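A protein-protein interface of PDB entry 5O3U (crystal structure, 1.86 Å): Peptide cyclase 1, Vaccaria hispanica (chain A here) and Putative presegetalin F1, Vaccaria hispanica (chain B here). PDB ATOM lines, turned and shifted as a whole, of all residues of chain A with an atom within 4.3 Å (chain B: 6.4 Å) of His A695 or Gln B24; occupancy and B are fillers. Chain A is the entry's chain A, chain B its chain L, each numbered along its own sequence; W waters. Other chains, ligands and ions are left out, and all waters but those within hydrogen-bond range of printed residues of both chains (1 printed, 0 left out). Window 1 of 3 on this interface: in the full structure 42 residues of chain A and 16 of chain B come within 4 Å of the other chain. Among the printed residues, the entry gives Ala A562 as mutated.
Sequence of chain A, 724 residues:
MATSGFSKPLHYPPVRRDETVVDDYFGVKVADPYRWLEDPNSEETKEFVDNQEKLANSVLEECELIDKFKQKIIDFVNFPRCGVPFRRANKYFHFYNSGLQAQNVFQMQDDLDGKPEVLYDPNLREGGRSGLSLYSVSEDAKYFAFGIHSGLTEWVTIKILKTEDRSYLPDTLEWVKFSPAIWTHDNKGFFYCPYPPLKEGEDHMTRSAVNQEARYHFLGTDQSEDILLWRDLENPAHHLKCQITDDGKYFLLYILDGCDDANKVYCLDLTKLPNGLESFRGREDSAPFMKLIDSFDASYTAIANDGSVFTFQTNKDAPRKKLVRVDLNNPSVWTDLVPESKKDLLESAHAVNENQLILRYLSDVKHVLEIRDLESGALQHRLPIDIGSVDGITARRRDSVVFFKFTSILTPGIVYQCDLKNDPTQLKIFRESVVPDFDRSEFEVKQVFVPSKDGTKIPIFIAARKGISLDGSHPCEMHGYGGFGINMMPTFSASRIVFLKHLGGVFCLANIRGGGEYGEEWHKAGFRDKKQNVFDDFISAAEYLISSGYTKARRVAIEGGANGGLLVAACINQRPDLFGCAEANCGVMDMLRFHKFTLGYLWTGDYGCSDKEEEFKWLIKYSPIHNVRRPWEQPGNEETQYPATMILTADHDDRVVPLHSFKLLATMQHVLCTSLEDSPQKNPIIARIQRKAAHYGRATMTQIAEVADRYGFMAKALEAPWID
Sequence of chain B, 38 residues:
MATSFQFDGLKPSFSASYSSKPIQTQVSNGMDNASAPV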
ATOM      1  N   GLU A 154      -0.384  10.837  24.468  1.00  0.00           N
ATOM      2  CA  GLU A 154      -1.241   9.810  23.882  1.00  0.00           C
ATOM      3  C   GLU A 154      -2.560   9.584  24.671  1.00  0.00           C
ATOM      4  O   GLU A 154      -3.383   8.740  24.285  1.00  0.00           O
ATOM      5  CB  GLU A 154      -0.461   8.484  23.814  1.00  0.00           C
ATOM      6  CG  GLU A 154       0.815   8.535  22.968  1.00  0.00           C
ATOM      7  CD  GLU A 154       0.717   7.784  21.643  1.00  0.00           C
ATOM      8  OE1 GLU A 154       0.323   6.603  21.616  1.00  0.00           O
ATOM      9  OE2 GLU A 154       1.050   8.382  20.613  1.00  0.00           O
ATOM     10  N   GLU A 559      12.689   4.981   1.931  1.00  0.00           N
ATOM     11  CA  GLU A 559      11.908   5.674   2.939  1.00  0.00           C
ATOM     12  C   GLU A 559      11.135   4.664   3.768  1.00  0.00           C
ATOM     13  O   GLU A 559      10.653   3.646   3.245  1.00  0.00           O
ATOM     14  CB  GLU A 559      10.935   6.679   2.312  1.00  0.00           C
ATOM     15  CG  GLU A 559      10.200   7.578   3.332  1.00  0.00           C
ATOM     16  CD  GLU A 559       8.905   7.002   3.936  1.00  0.00           C
ATOM     17  OE1 GLU A 559       8.204   6.193   3.272  1.00  0.00           O
ATOM     18  OE2 GLU A 559       8.584   7.369   5.097  1.00  0.00           O
ATOM     19  N   GLY A 561       9.084   4.337   8.055  1.00  0.00           N
ATOM     20  CA  GLY A 561       8.771   4.907   9.358  1.00  0.00           C
ATOM     21  C   GLY A 561       8.728   3.920  10.508  1.00  0.00           C
ATOM     22  O   GLY A 561       8.182   2.815  10.362  1.00  0.00           O
ATOM     23  N   ALA A 562       9.264   4.339  11.664  1.00  0.00           N
ATOM     24  CA  ALA A 562       9.267   3.555  12.923  1.00  0.00           C
ATOM     25  C   ALA A 562      10.107   2.279  12.788  1.00  0.00           C
ATOM     26  O   ALA A 562      11.317   2.377  12.610  1.00  0.00           O
ATOM     27  CB  ALA A 562       7.839   3.307  13.412  1.00  0.00           C
ATOM     28  N   ASN A 585      11.684   8.065   9.079  1.00  0.00           N
ATOM     29  CA  ASN A 585      10.724   8.749   9.901  1.00  0.00           C
ATOM     30  C   ASN A 585      10.577   8.010  11.256  1.00  0.00           C
ATOM     31  O   ASN A 585      10.345   6.800  11.276  1.00  0.00           O
ATOM     32  CB  ASN A 585       9.390   8.818   9.155  1.00  0.00           C
ATOM     33  CG  ASN A 585       8.545   9.992   9.614  1.00  0.00           C
ATOM     34  OD1 ASN A 585       8.414  10.238  10.805  1.00  0.00           O
ATOM     35  ND2 ASN A 585       8.002  10.751   8.672  1.00  0.00           N
ATOM     36  N   CYS A 586      10.759   8.739  12.353  1.00  0.00           N
ATOM     37  CA  CYS A 586      10.649   8.229  13.724  1.00  0.00           C
ATOM     38  C   CYS A 586      11.174   6.804  13.909  1.00  0.00           C
ATOM     39  O   CYS A 586      10.483   5.931  14.445  1.00  0.00           O
ATOM     40  CB  CYS A 586       9.200   8.351  14.237  1.00  0.00           C
ATOM     41  SG  CYS A 586       7.956   7.365  13.375  1.00  0.00           S
ATOM     42  N   ASP A 653       7.033  12.673  20.100  1.00  0.00           N
ATOM     43  CA  ASP A 653       6.555  11.334  19.758  1.00  0.00           C
ATOM     44  C   ASP A 653       6.712  10.458  21.019  1.00  0.00           C
ATOM     45  O   ASP A 653       7.823  10.248  21.492  1.00  0.00           O
ATOM     46  CB  ASP A 653       7.325  10.787  18.558  1.00  0.00           C
ATOM     47  CG  ASP A 653       6.693   9.525  17.972  1.00  0.00           C
ATOM     48  OD1 ASP A 653       6.121   8.689  18.739  1.00  0.00           O
ATOM     49  OD2 ASP A 653       6.798   9.342  16.735  1.00  0.00           O
ATOM     50  N   ARG A 655       5.389   7.288  21.050  1.00  0.00           N
ATOM     51  CA  ARG A 655       5.422   5.903  20.581  1.00  0.00           C
ATOM     52  C   ARG A 655       6.886   5.495  20.401  1.00  0.00           C
ATOM     53  O   ARG A 655       7.350   4.548  21.028  1.00  0.00           O
ATOM     54  CB  ARG A 655       4.635   5.751  19.267  1.00  0.00           C
ATOM     55  CG  ARG A 655       4.558   4.314  18.708  1.00  0.00           C
ATOM     56  CD  ARG A 655       3.675   3.391  19.541  1.00  0.00           C
ATOM     57  NE  ARG A 655       2.296   3.880  19.524  1.00  0.00           N
ATOM     58  CZ  ARG A 655       1.353   3.537  18.646  1.00  0.00           C
ATOM     59  NH1 ARG A 655       1.582   2.628  17.713  1.00  0.00           N
ATOM     60  NH2 ARG A 655       0.158   4.088  18.712  1.00  0.00           N
ATOM     61  N   ALA A 694       2.871  15.247  18.069  1.00  0.00           N
ATOM     62  CA  ALA A 694       2.835  13.949  18.717  1.00  0.00           C
ATOM     63  C   ALA A 694       2.998  12.892  17.639  1.00  0.00           C
ATOM     64  O   ALA A 694       3.201  13.207  16.472  1.00  0.00           O
ATOM     65  CB  ALA A 694       1.498  13.777  19.417  1.00  0.00           C
ATOM     66  N   HIS A 695       2.907  11.630  18.039  1.00  0.00           N
ATOM     67  CA  HIS A 695       2.877  10.544  17.077  1.00  0.00           C
ATOM     68  C   HIS A 695       1.635  10.554  16.185  1.00  0.00           C
ATOM     69  O   HIS A 695       1.717  10.251  15.003  1.00  0.00           O
ATOM     70  CB  HIS A 695       2.974   9.192  17.779  1.00  0.00           C
ATOM     71  CG  HIS A 695       3.159   8.053  16.831  1.00  0.00           C
ATOM     72  ND1 HIS A 695       4.328   7.865  16.115  1.00  0.00           N
ATOM     73  CD2 HIS A 695       2.308   7.075  16.441  1.00  0.00           C
ATOM     74  CE1 HIS A 695       4.191   6.805  15.340  1.00  0.00           C
ATOM     75  NE2 HIS A 695       2.975   6.307  15.519  1.00  0.00           N
ATOM     76  N   TYR A 696       0.504  10.923  16.746  1.00  0.00           N
ATOM     77  CA  TYR A 696      -0.800  10.692  16.082  1.00  0.00           C
ATOM     78  C   TYR A 696      -1.142  11.785  15.102  1.00  0.00           C
ATOM     79  O   TYR A 696      -0.505  12.847  15.097  1.00  0.00           O
ATOM     80  CB  TYR A 696      -1.930  10.528  17.086  1.00  0.00           C
ATOM     81  CG  TYR A 696      -1.920  11.552  18.183  1.00  0.00           C
ATOM     82  CD1 TYR A 696      -2.554  12.793  18.052  1.00  0.00           C
ATOM     83  CD2 TYR A 696      -1.262  11.271  19.376  1.00  0.00           C
ATOM     84  CE1 TYR A 696      -2.556  13.699  19.089  1.00  0.00           C
ATOM     85  CE2 TYR A 696      -1.229  12.188  20.405  1.00  0.00           C
ATOM     86  CZ  TYR A 696      -1.879  13.398  20.257  1.00  0.00           C
ATOM     87  OH  TYR A 696      -1.886  14.293  21.304  1.00  0.00           O
ATOM     88  N   GLY A 697      -2.166  11.477  14.295  1.00  0.00           N
ATOM     89  CA  GLY A 697      -2.469  12.092  12.995  1.00  0.00           C
ATOM     90  C   GLY A 697      -2.484  13.602  12.759  1.00  0.00           C
ATOM     91  O   GLY A 697      -3.474  14.326  13.017  1.00  0.00           O
ATOM     92  N   LYS B  21       2.490  -1.389  18.433  1.00  0.00           N
ATOM     93  CA  LYS B  21       3.623  -1.572  17.530  1.00  0.00           C
ATOM     94  C   LYS B  21       4.348  -0.272  17.153  1.00  0.00           C
ATOM     95  O   LYS B  21       3.743   0.796  17.162  1.00  0.00           O
ATOM     96  CB  LYS B  21       3.156  -2.295  16.275  1.00  0.00           C
ATOM     97  CG  LYS B  21       2.708  -3.711  16.592  1.00  0.00           C
ATOM     98  CD  LYS B  21       1.862  -4.303  15.495  1.00  0.00           C
ATOM     99  CE  LYS B  21       1.470  -5.714  15.914  1.00  0.00           C
ATOM    100  NZ  LYS B  21       0.730  -6.339  14.799  1.00  0.00           N
ATOM    101  N   PRO B  22       5.643  -0.378  16.802  1.00  0.00           N
ATOM    102  CA  PRO B  22       6.363   0.807  16.311  1.00  0.00           C
ATOM    103  C   PRO B  22       5.999   1.022  14.829  1.00  0.00           C
ATOM    104  O   PRO B  22       6.650   0.507  13.910  1.00  0.00           O
ATOM    105  CB  PRO B  22       7.827   0.429  16.526  1.00  0.00           C
ATOM    106  CG  PRO B  22       7.872  -1.047  16.423  1.00  0.00           C
ATOM    107  CD  PRO B  22       6.491  -1.587  16.752  1.00  0.00           C
ATOM    108  N   ILE B  23       4.920   1.762  14.613  1.00  0.00           N
ATOM    109  CA  ILE B  23       4.397   1.997  13.276  1.00  0.00           C
ATOM    110  C   ILE B  23       3.819   3.404  13.239  1.00  0.00           C
ATOM    111  O   ILE B  23       3.381   3.903  14.273  1.00  0.00           O
ATOM    112  CB  ILE B  23       3.359   0.914  12.880  1.00  0.00           C
ATOM    113  CG1 ILE B  23       3.029   1.022  11.385  1.00  0.00           C
ATOM    114  CG2 ILE B  23       2.113   0.971  13.770  1.00  0.00           C
ATOM    115  CD1 ILE B  23       2.162  -0.100  10.849  1.00  0.00           C
ATOM    116  N   GLN B  24       3.859   4.054  12.074  1.00  0.00           N
ATOM    117  CA  GLN B  24       3.298   5.417  11.908  1.00  0.00           C
ATOM    118  C   GLN B  24       2.017   5.370  11.061  1.00  0.00           C
ATOM    119  O   GLN B  24       1.284   4.399  11.137  1.00  0.00           O
ATOM    120  CB  GLN B  24       4.353   6.362  11.329  1.00  0.00           C
ATOM    121  CG  GLN B  24       4.882   6.026   9.937  1.00  0.00           C
ATOM    122  CD  GLN B  24       5.731   7.135   9.323  1.00  0.00           C
ATOM    123  OE1 GLN B  24       5.952   8.187   9.934  1.00  0.00           O
ATOM    124  NE2 GLN B  24       6.233   6.893   8.103  1.00  0.00           N
ATOM    125  N   THR B  25       1.681   6.433  10.316  1.00  0.00           N
ATOM    126  CA  THR B  25       0.849   6.298   9.085  1.00  0.00           C
ATOM    127  C   THR B  25       1.164   7.420   8.077  1.00  0.00           C
ATOM    128  O   THR B  25       0.396   8.370   7.893  1.00  0.00           O
ATOM    129  CB  THR B  25      -0.681   6.206   9.357  1.00  0.00           C
ATOM    130  OG1 THR B  25      -0.945   5.256  10.398  1.00  0.00           O
ATOM    131  CG2 THR B  25      -1.447   5.765   8.075  1.00  0.00           C
HETATM  132  O   HOH W   1       5.473   2.843   9.760  1.00  0.00           O
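The side-chain amide oxygen (OD1) of Asn A585 lies close to the side-chain amide oxygen (OE1) of Gln B24 (3.3 Å).
The guanidinium group (NH1) of Arg A655 lies within hydrogen-bond range of the backbone carbonyl oxygen (O) of Lys B21 (2.9 Å).
A ring nitrogen (NE2) of His A695 lies within hydrogen-bond range of the backbone carbonyl oxygen (O) of Ile B23.
His A695 touches two residues of chain B.
Gln B24 touches just these residues of chain A: Glu A559 (3.8 Å), Gly A561 (3.5 Å), Asn A585 (3.2 Å) and His A695 (3.7 Å).
Printed residues of chain B within 4 Å of Glu A559: Gln B24.
Printed residues of chain A within 4 Å of Ile B23: Ala A562 (3.5 Å) and His A695 (2.7 Å).
Of the printed residues of chain B, Ala A562 touches Pro B22 and Ile B23.
Of the printed residues of chain B, Arg A655 touches Lys B21.
Ala A694 touches none of the printed residues of chain B.
Gly A697 touches none of the printed residues of chain B.
OE1 of Glu A154 is in salt-bridge range of NH2 of Arg A655 (3.8 Å).
The backbone NH (N) of Ala A562 lies within hydrogen-bond range of the backbone carbonyl oxygen (O) of Asn A585, at 2.7 Å.
The backbone carbonyl oxygen (O) of Cys A586 lies close to the backbone NH (N) of Ala A562.
The side-chain carboxylate (OD1) of Asp A653 sits at hydrogen-bond distance from the backbone NH (N) of Arg A655, 2.8 Å away.
A ring nitrogen (ND1) of His A695 is in hydrogen-bond range of the side-chain carboxylate (OD2) of Asp A653, 2.9 Å away.
OE2 of Glu A559 touches NE2 of Gln B24 (3.8 Å).
Gly A561 touches Gln B24 (CA to NE2, 3.5 Å).
O of Pro B22 touches CB of Ala A562 (3.1 Å).
Ala A562 touches Ile B23.
His A695 touches Gln B24.
Water W1 lies within hydrogen-bond range of the backbone carbonyl oxygen (O) of Gly A561 and the backbone NH (N) of Gln B24.
Of the 12 printed residues of chain A, 6 touch a printed residue of chain B.
Printed residues of chain A that touch a printed residue of chain B: Glu A559, Gly A561, Ala A562, Asn A585, Arg A655 and His A695.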
